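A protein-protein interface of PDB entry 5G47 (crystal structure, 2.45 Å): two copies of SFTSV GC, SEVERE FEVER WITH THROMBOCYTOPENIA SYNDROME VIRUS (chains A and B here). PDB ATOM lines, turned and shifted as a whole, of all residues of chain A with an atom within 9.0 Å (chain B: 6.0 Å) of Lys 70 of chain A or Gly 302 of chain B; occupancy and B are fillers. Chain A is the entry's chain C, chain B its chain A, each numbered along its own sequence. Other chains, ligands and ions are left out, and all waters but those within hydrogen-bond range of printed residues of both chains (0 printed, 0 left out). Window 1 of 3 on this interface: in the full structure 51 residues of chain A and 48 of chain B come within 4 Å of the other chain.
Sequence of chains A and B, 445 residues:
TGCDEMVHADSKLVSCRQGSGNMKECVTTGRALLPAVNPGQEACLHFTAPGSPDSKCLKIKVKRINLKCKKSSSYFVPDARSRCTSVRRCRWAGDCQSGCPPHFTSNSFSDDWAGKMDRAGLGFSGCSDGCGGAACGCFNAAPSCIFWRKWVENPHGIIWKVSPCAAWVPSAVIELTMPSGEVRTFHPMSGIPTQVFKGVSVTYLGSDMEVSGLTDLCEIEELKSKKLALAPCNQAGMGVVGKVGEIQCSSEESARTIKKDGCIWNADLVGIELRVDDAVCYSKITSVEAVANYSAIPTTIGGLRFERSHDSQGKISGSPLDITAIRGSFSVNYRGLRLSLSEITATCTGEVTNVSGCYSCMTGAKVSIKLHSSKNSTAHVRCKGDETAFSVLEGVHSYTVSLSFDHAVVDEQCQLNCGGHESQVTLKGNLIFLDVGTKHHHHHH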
ATOM      1  N   LEU A  67       2.748 -15.956   4.147  1.00  0.00           N
ATOM      2  CA  LEU A  67       4.155 -16.199   4.439  1.00  0.00           C
ATOM      3  C   LEU A  67       4.619 -17.389   3.612  1.00  0.00           C
ATOM      4  O   LEU A  67       4.040 -18.477   3.702  1.00  0.00           O
ATOM      5  CB  LEU A  67       4.366 -16.463   5.928  1.00  0.00           C
ATOM      6  CG  LEU A  67       3.924 -15.353   6.881  1.00  0.00           C
ATOM      7  CD1 LEU A  67       4.129 -15.795   8.320  1.00  0.00           C
ATOM      8  CD2 LEU A  67       4.674 -14.060   6.590  1.00  0.00           C
ATOM      9  N   LYS A  68       5.649 -17.180   2.799  1.00  0.00           N
ATOM     10  CA  LYS A  68       6.156 -18.201   1.895  1.00  0.00           C
ATOM     11  C   LYS A  68       7.486 -18.732   2.409  1.00  0.00           C
ATOM     12  O   LYS A  68       8.372 -17.954   2.780  1.00  0.00           O
ATOM     13  CB  LYS A  68       6.312 -17.648   0.477  1.00  0.00           C
ATOM     14  CG  LYS A  68       4.985 -17.412  -0.228  1.00  0.00           C
ATOM     15  CD  LYS A  68       4.147 -18.687  -0.244  1.00  0.00           C
ATOM     16  CE  LYS A  68       2.766 -18.441  -0.829  1.00  0.00           C
ATOM     17  NZ  LYS A  68       1.956 -19.687  -0.903  1.00  0.00           N
ATOM     18  N   CYS A  69       7.615 -20.053   2.434  1.00  0.00           N
ATOM     19  CA  CYS A  69       8.847 -20.690   2.878  1.00  0.00           C
ATOM     20  C   CYS A  69       9.944 -20.473   1.843  1.00  0.00           C
ATOM     21  O   CYS A  69       9.832 -20.942   0.706  1.00  0.00           O
ATOM     22  CB  CYS A  69       8.601 -22.180   3.101  1.00  0.00           C
ATOM     23  SG  CYS A  69      10.073 -23.208   3.302  1.00  0.00           S
ATOM     24  N   LYS A  70      10.994 -19.751   2.229  1.00  0.00           N
ATOM     25  CA  LYS A  70      12.167 -19.566   1.377  1.00  0.00           C
ATOM     26  C   LYS A  70      13.136 -20.700   1.687  1.00  0.00           C
ATOM     27  O   LYS A  70      13.839 -20.675   2.701  1.00  0.00           O
ATOM     28  CB  LYS A  70      12.797 -18.196   1.607  1.00  0.00           C
ATOM     29  CG  LYS A  70      13.841 -17.825   0.571  1.00  0.00           C
ATOM     30  CD  LYS A  70      13.266 -17.899  -0.835  1.00  0.00           C
ATOM     31  CE  LYS A  70      14.338 -17.679  -1.888  1.00  0.00           C
ATOM     32  NZ  LYS A  70      13.802 -17.846  -3.268  1.00  0.00           N
ATOM     33  N   LYS A  71      13.172 -21.697   0.808  1.00  0.00           N
ATOM     34  CA  LYS A  71      13.831 -22.958   1.106  1.00  0.00           C
ATOM     35  C   LYS A  71      15.346 -22.852   0.992  1.00  0.00           C
ATOM     36  O   LYS A  71      15.885 -22.043   0.232  1.00  0.00           O
ATOM     37  CB  LYS A  71      13.341 -24.056   0.163  1.00  0.00           C
ATOM     38  CG  LYS A  71      11.834 -24.217   0.108  1.00  0.00           C
ATOM     39  CD  LYS A  71      11.451 -25.253  -0.937  1.00  0.00           C
ATOM     40  CE  LYS A  71       9.945 -25.415  -1.024  1.00  0.00           C
ATOM     41  NZ  LYS A  71       9.275 -24.142  -1.414  1.00  0.00           N
ATOM     42  N   SER A  72      16.030 -23.690   1.762  1.00  0.00           N
ATOM     43  CA  SER A  72      17.444 -23.958   1.542  1.00  0.00           C
ATOM     44  C   SER A  72      17.551 -25.243   0.715  1.00  0.00           C
ATOM     45  O   SER A  72      16.573 -25.666   0.094  1.00  0.00           O
ATOM     46  CB  SER A  72      18.179 -24.018   2.883  1.00  0.00           C
ATOM     47  OG  SER A  72      17.549 -24.922   3.768  1.00  0.00           O
ATOM     48  N   SER A  73      18.718 -25.882   0.691  1.00  0.00           N
ATOM     49  CA  SER A  73      18.894 -27.069  -0.139  1.00  0.00           C
ATOM     50  C   SER A  73      18.016 -28.213   0.358  1.00  0.00           C
ATOM     51  O   SER A  73      17.952 -28.485   1.560  1.00  0.00           O
ATOM     52  CB  SER A  73      20.363 -27.489  -0.152  1.00  0.00           C
ATOM     53  OG  SER A  73      21.186 -26.459  -0.681  1.00  0.00           O
ATOM     54  N   SER A  74      17.341 -28.882  -0.569  1.00  0.00           N
ATOM     55  CA  SER A  74      16.462 -29.993  -0.239  1.00  0.00           C
ATOM     56  C   SER A  74      17.239 -31.304  -0.171  1.00  0.00           C
ATOM     57  O   SER A  74      18.307 -31.463  -0.769  1.00  0.00           O
ATOM     58  CB  SER A  74      15.335 -30.117  -1.265  1.00  0.00           C
ATOM     59  OG  SER A  74      14.571 -28.925  -1.354  1.00  0.00           O
ATOM     60  N   SER A 163      12.643 -29.926   2.939  1.00  0.00           N
ATOM     61  CA  SER A 163      13.155 -28.626   2.510  1.00  0.00           C
ATOM     62  C   SER A 163      13.122 -27.677   3.700  1.00  0.00           C
ATOM     63  O   SER A 163      12.046 -27.174   4.067  1.00  0.00           O
ATOM     64  CB  SER A 163      12.340 -28.070   1.348  1.00  0.00           C
ATOM     65  OG  SER A 163      12.262 -29.008   0.288  1.00  0.00           O
ATOM     66  N   PRO A 164      14.265 -27.416   4.334  1.00  0.00           N
ATOM     67  CA  PRO A 164      14.281 -26.463   5.449  1.00  0.00           C
ATOM     68  C   PRO A 164      13.896 -25.067   4.982  1.00  0.00           C
ATOM     69  O   PRO A 164      14.285 -24.624   3.899  1.00  0.00           O
ATOM     70  CB  PRO A 164      15.732 -26.510   5.940  1.00  0.00           C
ATOM     71  CG  PRO A 164      16.271 -27.811   5.437  1.00  0.00           C
ATOM     72  CD  PRO A 164      15.577 -28.054   4.130  1.00  0.00           C
ATOM     73  N   CYS A 165      13.122 -24.375   5.813  1.00  0.00           N
ATOM     74  CA  CYS A 165      12.717 -23.000   5.529  1.00  0.00           C
ATOM     75  C   CYS A 165      13.737 -22.069   6.173  1.00  0.00           C
ATOM     76  O   CYS A 165      13.678 -21.800   7.375  1.00  0.00           O
ATOM     77  CB  CYS A 165      11.306 -22.732   6.041  1.00  0.00           C
ATOM     78  SG  CYS A 165      10.042 -23.755   5.260  1.00  0.00           S
ATOM     79  N   ALA A 166      14.684 -21.583   5.369  1.00  0.00           N
ATOM     80  CA  ALA A 166      15.701 -20.677   5.891  1.00  0.00           C
ATOM     81  C   ALA A 166      15.098 -19.353   6.339  1.00  0.00           C
ATOM     82  O   ALA A 166      15.657 -18.683   7.216  1.00  0.00           O
ATOM     83  CB  ALA A 166      16.785 -20.439   4.839  1.00  0.00           C
ATOM     84  N   ALA A 167      13.966 -18.963   5.758  1.00  0.00           N
ATOM     85  CA  ALA A 167      13.309 -17.710   6.107  1.00  0.00           C
ATOM     86  C   ALA A 167      11.887 -17.737   5.561  1.00  0.00           C
ATOM     87  O   ALA A 167      11.496 -18.656   4.835  1.00  0.00           O
ATOM     88  CB  ALA A 167      14.080 -16.503   5.566  1.00  0.00           C
ATOM     89  N   TRP A 168      11.117 -16.711   5.922  1.00  0.00           N
ATOM     90  CA  TRP A 168       9.734 -16.566   5.487  1.00  0.00           C
ATOM     91  C   TRP A 168       9.526 -15.164   4.935  1.00  0.00           C
ATOM     92  O   TRP A 168       9.971 -14.181   5.533  1.00  0.00           O
ATOM     93  CB  TRP A 168       8.757 -16.841   6.642  1.00  0.00           C
ATOM     94  CG  TRP A 168       8.828 -18.251   7.149  1.00  0.00           C
ATOM     95  CD1 TRP A 168       9.713 -18.750   8.059  1.00  0.00           C
ATOM     96  CD2 TRP A 168       7.986 -19.349   6.767  1.00  0.00           C
ATOM     97  NE1 TRP A 168       9.475 -20.086   8.270  1.00  0.00           N
ATOM     98  CE2 TRP A 168       8.420 -20.478   7.489  1.00  0.00           C
ATOM     99  CE3 TRP A 168       6.907 -19.485   5.887  1.00  0.00           C
ATOM    100  CZ2 TRP A 168       7.814 -21.727   7.359  1.00  0.00           C
ATOM    101  CZ3 TRP A 168       6.308 -20.726   5.759  1.00  0.00           C
ATOM    102  CH2 TRP A 168       6.763 -21.830   6.491  1.00  0.00           C
ATOM    103  N   VAL A 169       8.852 -15.077   3.793  1.00  0.00           N
ATOM    104  CA  VAL A 169       8.679 -13.809   3.086  1.00  0.00           C
ATOM    105  C   VAL A 169       7.194 -13.544   2.866  1.00  0.00           C
ATOM    106  O   VAL A 169       6.463 -14.443   2.424  1.00  0.00           O
ATOM    107  CB  VAL A 169       9.448 -13.810   1.754  1.00  0.00           C
ATOM    108  CG1 VAL A 169       9.108 -12.575   0.935  1.00  0.00           C
ATOM    109  CG2 VAL A 169      10.947 -13.890   2.008  1.00  0.00           C
ATOM    110  N   PRO A 170       6.703 -12.343   3.169  1.00  0.00           N
ATOM    111  CA  PRO A 170       5.288 -12.042   2.926  1.00  0.00           C
ATOM    112  C   PRO A 170       4.989 -11.935   1.439  1.00  0.00           C
ATOM    113  O   PRO A 170       5.752 -11.345   0.671  1.00  0.00           O
ATOM    114  CB  PRO A 170       5.082 -10.695   3.632  1.00  0.00           C
ATOM    115  CG  PRO A 170       6.262 -10.550   4.561  1.00  0.00           C
ATOM    116  CD  PRO A 170       7.386 -11.253   3.879  1.00  0.00           C
ATOM    117  N   LEU A 217      11.745 -24.208  10.954  1.00  0.00           N
ATOM    118  CA  LEU A 217      10.799 -25.197  10.465  1.00  0.00           C
ATOM    119  C   LEU A 217      11.237 -25.688   9.092  1.00  0.00           C
ATOM    120  O   LEU A 217      11.993 -25.022   8.382  1.00  0.00           O
ATOM    121  CB  LEU A 217       9.378 -24.618  10.393  1.00  0.00           C
ATOM    122  CG  LEU A 217       8.762 -24.196  11.729  1.00  0.00           C
ATOM    123  CD1 LEU A 217       7.438 -23.479  11.515  1.00  0.00           C
ATOM    124  CD2 LEU A 217       8.581 -25.403  12.634  1.00  0.00           C
ATOM    125  N   CYS A 218      10.744 -26.869   8.724  1.00  0.00           N
ATOM    126  CA  CYS A 218      11.089 -27.493   7.456  1.00  0.00           C
ATOM    127  C   CYS A 218       9.840 -28.056   6.802  1.00  0.00           C
ATOM    128  O   CYS A 218       8.975 -28.619   7.479  1.00  0.00           O
ATOM    129  CB  CYS A 218      12.112 -28.618   7.639  1.00  0.00           C
ATOM    130  SG  CYS A 218      13.601 -28.178   8.554  1.00  0.00           S
ATOM    131  N   GLU A 219       9.760 -27.917   5.482  1.00  0.00           N
ATOM    132  CA  GLU A 219       8.676 -28.513   4.711  1.00  0.00           C
ATOM    133  C   GLU A 219       8.973 -29.989   4.479  1.00  0.00           C
ATOM    134  O   GLU A 219      10.012 -30.338   3.909  1.00  0.00           O
ATOM    135  CB  GLU A 219       8.503 -27.778   3.386  1.00  0.00           C
ATOM    136  CG  GLU A 219       7.526 -28.445   2.435  1.00  0.00           C
ATOM    137  CD  GLU A 219       7.362 -27.676   1.142  1.00  0.00           C
ATOM    138  OE1 GLU A 219       7.637 -26.458   1.139  1.00  0.00           O
ATOM    139  OE2 GLU A 219       6.964 -28.289   0.129  1.00  0.00           O
ATOM    140  N   GLN A 235      19.660 -29.134   8.655  1.00  0.00           N
ATOM    141  CA  GLN A 235      20.027 -28.575   7.366  1.00  0.00           C
ATOM    142  C   GLN A 235      20.565 -29.680   6.462  1.00  0.00           C
ATOM    143  O   GLN A 235      20.908 -30.776   6.913  1.00  0.00           O
ATOM    144  CB  GLN A 235      21.074 -27.473   7.530  1.00  0.00           C
ATOM    145  CG  GLN A 235      20.665 -26.368   8.486  1.00  0.00           C
ATOM    146  CD  GLN A 235      19.498 -25.555   7.970  1.00  0.00           C
ATOM    147  OE1 GLN A 235      18.488 -25.394   8.653  1.00  0.00           O
ATOM    148  NE2 GLN A 235      19.634 -25.030   6.757  1.00  0.00           N
ATOM    149  N   GLN A 313       4.285 -20.735  -5.907  1.00  0.00           N
ATOM    150  CA  GLN A 313       5.569 -20.349  -5.335  1.00  0.00           C
ATOM    151  C   GLN A 313       5.718 -20.893  -3.919  1.00  0.00           C
ATOM    152  O   GLN A 313       5.996 -20.137  -2.984  1.00  0.00           O
ATOM    153  CB  GLN A 313       5.723 -18.824  -5.339  1.00  0.00           C
ATOM    154  CG  GLN A 313       5.962 -18.213  -6.715  1.00  0.00           C
ATOM    155  CD  GLN A 313       4.742 -18.273  -7.618  1.00  0.00           C
ATOM    156  OE1 GLN A 313       3.633 -18.561  -7.167  1.00  0.00           O
ATOM    157  NE2 GLN A 313       4.943 -18.002  -8.903  1.00  0.00           N
ATOM    158  N   GLY A 314       5.545 -22.200  -3.755  1.00  0.00           N
ATOM    159  CA  GLY A 314       5.598 -22.813  -2.431  1.00  0.00           C
ATOM    160  C   GLY A 314       4.279 -23.493  -2.120  1.00  0.00           C
ATOM    161  O   GLY A 314       3.202 -22.919  -2.268  1.00  0.00           O
ATOM    162  N   ILE A 316       3.273 -24.418   0.803  1.00  0.00           N
ATOM    163  CA  ILE A 316       2.809 -24.041   2.132  1.00  0.00           C
ATOM    164  C   ILE A 316       2.780 -22.522   2.224  1.00  0.00           C
ATOM    165  O   ILE A 316       3.727 -21.848   1.804  1.00  0.00           O
ATOM    166  CB  ILE A 316       3.708 -24.637   3.236  1.00  0.00           C
ATOM    167  CG1 ILE A 316       3.619 -26.164   3.238  1.00  0.00           C
ATOM    168  CG2 ILE A 316       3.338 -24.072   4.601  1.00  0.00           C
ATOM    169  CD1 ILE A 316       4.533 -26.829   4.253  1.00  0.00           C
ATOM    170  N   VAL B 211      11.659 -10.031   5.313  1.00  0.00           N
ATOM    171  CA  VAL B 211      12.166 -11.375   5.566  1.00  0.00           C
ATOM    172  C   VAL B 211      12.209 -11.612   7.070  1.00  0.00           C
ATOM    173  O   VAL B 211      12.829 -10.847   7.818  1.00  0.00           O
ATOM    174  CB  VAL B 211      13.547 -11.571   4.930  1.00  0.00           C
ATOM    175  CG1 VAL B 211      14.034 -12.993   5.144  1.00  0.00           C
ATOM    176  CG2 VAL B 211      13.507 -11.230   3.448  1.00  0.00           C
ATOM    177  N   LEU B 214      14.557 -15.842  10.086  1.00  0.00           N
ATOM    178  CA  LEU B 214      15.820 -16.318   9.533  1.00  0.00           C
ATOM    179  C   LEU B 214      16.442 -17.389  10.419  1.00  0.00           C
ATOM    180  O   LEU B 214      16.471 -17.264  11.645  1.00  0.00           O
ATOM    181  CB  LEU B 214      16.793 -15.150   9.359  1.00  0.00           C
ATOM    182  CG  LEU B 214      18.151 -15.491   8.743  1.00  0.00           C
ATOM    183  CD1 LEU B 214      17.965 -16.160   7.389  1.00  0.00           C
ATOM    184  CD2 LEU B 214      19.009 -14.243   8.611  1.00  0.00           C
ATOM    185  N   THR B 300      24.413 -16.945  -0.221  1.00  0.00           N
ATOM    186  CA  THR B 300      23.007 -16.560  -0.259  1.00  0.00           C
ATOM    187  C   THR B 300      22.192 -17.551   0.561  1.00  0.00           C
ATOM    188  O   THR B 300      22.211 -18.754   0.279  1.00  0.00           O
ATOM    189  CB  THR B 300      22.491 -16.501  -1.697  1.00  0.00           C
ATOM    190  OG1 THR B 300      23.093 -15.391  -2.377  1.00  0.00           O
ATOM    191  CG2 THR B 300      20.981 -16.345  -1.715  1.00  0.00           C
ATOM    192  N   ILE B 301      21.477 -17.045   1.565  1.00  0.00           N
ATOM    193  CA  ILE B 301      20.678 -17.868   2.470  1.00  0.00           C
ATOM    194  C   ILE B 301      19.316 -17.215   2.660  1.00  0.00           C
ATOM    195  O   ILE B 301      19.233 -16.039   3.028  1.00  0.00           O
ATOM    196  CB  ILE B 301      21.362 -18.062   3.838  1.00  0.00           C
ATOM    197  CG1 ILE B 301      22.769 -18.635   3.675  1.00  0.00           C
ATOM    198  CG2 ILE B 301      20.525 -18.972   4.727  1.00  0.00           C
ATOM    199  CD1 ILE B 301      23.527 -18.730   4.977  1.00  0.00           C
ATOM    200  N   GLY B 302      18.255 -17.980   2.426  1.00  0.00           N
ATOM    201  CA  GLY B 302      16.890 -17.520   2.632  1.00  0.00           C
ATOM    202  C   GLY B 302      16.529 -16.214   1.957  1.00  0.00           C
ATOM    203  O   GLY B 302      15.887 -15.355   2.578  1.00  0.00           O
ATOM    204  N   GLY B 303      16.919 -16.039   0.695  1.00  0.00           N
ATOM    205  CA  GLY B 303      16.647 -14.807  -0.017  1.00  0.00           C
ATOM    206  C   GLY B 303      17.562 -13.651   0.321  1.00  0.00           C
ATOM    207  O   GLY B 303      17.390 -12.564  -0.243  1.00  0.00           O
ATOM    208  N   LEU B 304      18.528 -13.845   1.215  1.00  0.00           N
ATOM    209  CA  LEU B 304      19.462 -12.803   1.611  1.00  0.00           C
ATOM    210  C   LEU B 304      20.855 -13.142   1.104  1.00  0.00           C
ATOM    211  O   LEU B 304      21.298 -14.289   1.204  1.00  0.00           O
ATOM    212  CB  LEU B 304      19.501 -12.646   3.132  1.00  0.00           C
ATOM    213  CG  LEU B 304      18.144 -12.532   3.823  1.00  0.00           C
ATOM    214  CD1 LEU B 304      18.307 -12.255   5.310  1.00  0.00           C
ATOM    215  CD2 LEU B 304      17.320 -11.456   3.149  1.00  0.00           C
ATOM    216  N   MET B 362      20.245 -23.884  -1.871  1.00  0.00           N
ATOM    217  CA  MET B 362      20.212 -22.731  -0.980  1.00  0.00           C
ATOM    218  C   MET B 362      20.477 -21.434  -1.734  1.00  0.00           C
ATOM    219  O   MET B 362      19.831 -20.413  -1.471  1.00  0.00           O
ATOM    220  CB  MET B 362      21.231 -22.921   0.143  1.00  0.00           C
ATOM    221  CG  MET B 362      21.313 -21.772   1.131  1.00  0.00           C
ATOM    222  SD  MET B 362      22.612 -22.020   2.358  1.00  0.00           S
ATOM    223  CE  MET B 362      24.062 -22.083   1.308  1.00  0.00           C
ATOM    224  N   ASP B 386       9.091 -18.425  -9.370  1.00  0.00           N
ATOM    225  CA  ASP B 386       9.737 -17.513  -8.435  1.00  0.00           C
ATOM    226  C   ASP B 386       9.656 -16.094  -8.984  1.00  0.00           C
ATOM    227  O   ASP B 386       9.246 -15.868 -10.125  1.00  0.00           O
ATOM    228  CB  ASP B 386      11.189 -17.935  -8.176  1.00  0.00           C
ATOM    229  CG  ASP B 386      11.767 -17.310  -6.921  1.00  0.00           C
ATOM    230  OD1 ASP B 386      10.991 -16.732  -6.130  1.00  0.00           O
ATOM    231  OD2 ASP B 386      12.997 -17.403  -6.723  1.00  0.00           O
ATOM    232  N   SER B 404      14.926 -19.078  -8.183  1.00  0.00           N
ATOM    233  CA  SER B 404      14.866 -20.446  -7.688  1.00  0.00           C
ATOM    234  C   SER B 404      14.034 -21.317  -8.619  1.00  0.00           C
ATOM    235  O   SER B 404      12.979 -20.899  -9.104  1.00  0.00           O
ATOM    236  CB  SER B 404      14.282 -20.493  -6.275  1.00  0.00           C
ATOM    237  OG  SER B 404      15.154 -19.880  -5.342  1.00  0.00           O
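Among the printed residues, merely in contact across the chains: Ala 166 of chain A with Leu 214 of chain B (3.3 Å), Lys 70 of chain A with Gly 302 of chain B (3.4 Å), Ala 167 of chain A with Val 211 of chain B (3.5 Å), Lys 70 of chain A with Gly 303 of chain B (3.6 Å), Trp 168 of chain A with Val 211 of chain B (3.6 Å), Ala 166 of chain A with Gly 302 of chain B (3.7 Å), Ala 167 of chain A with Gly 302 of chain B (3.7 Å), Ser 72 of chain A with Met 362 of chain B (3.9 Å) and Val 169 of chain A with Val 211 of chain B (3.96 Å).
No position is printed for both chains.
Printed residues of chain A that touch a printed residue of chain B: Lys 70, Ser 72, Ser 73, Ala 166, Ala 167, Trp 168 and Val 169.
Hydrophobic or aromatic side chains of chain B within 4 Å of the printed part of chain A: Val 211, Leu 214 and Met 362.
Along chain B the printed residues that touch a printed residue of chain A span positions 211 to 404.
Lys 70 of chain A touches just these residues of chain B: Gly 302 (3.4 Å), Gly 303 (3.6 Å), Asp 386 (3.6 Å) and Ser 404 (3.2 Å).
Of the printed residues of chain B, Ala 167 of chain A touches Val 211 (3.5 Å) and Gly 302 (3.7 Å).
Of chain A, only Lys 70, Ala 166 and Ala 167 come within 4 Å of Gly 302 of chain B.
Of chain A, only Lys 70 (3.6 Å) comes within 4 Å of Gly 303 of chain B.
Of the printed residues of chain A, Asp 386 of chain B touches Lys 70.
The nearest residue of chain B that does not touch Lys 70 of chain A is Ile 301 of chain B (5.9 Å).
OD2 of Asp 386 of chain B is in salt-bridge range of NZ of Lys 70 of chain A (3.6 Å).
The backbone NH (N) of Met 362 of chain B sits at hydrogen-bond distance from the side-chain hydroxyl (OG) of Ser 73 of chain A (3.0 Å).
The side-chain hydroxyl (OG) of Ser 404 of chain B lies within hydrogen-bond range of the side-chain amino group (NZ) of Lys 70 of chain A (3.2 Å).
The backbone carbonyl oxygen (O) of Lys 70 of chain A sits at hydrogen-bond distance from the backbone NH (N) of Ala 166 of chain A.
O of Val 169 of chain A sits at hydrogen-bond distance from N of Lys 68 of chain A (2.9 Å).
SG of Cys 69 of chain A forms a disulfide with SG of Cys 165 of chain A (2.0 Å).
OD2 of Asp 386 of chain B sits at hydrogen-bond distance from N of Ser 404 of chain B, 2.9 Å away.
N of Ser 72 of chain A lies within hydrogen-bond range of O of Pro 164 of chain A.
O of Ala 167 of chain A is in hydrogen-bond range of N of Lys 70 of chain A (2.9 Å).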
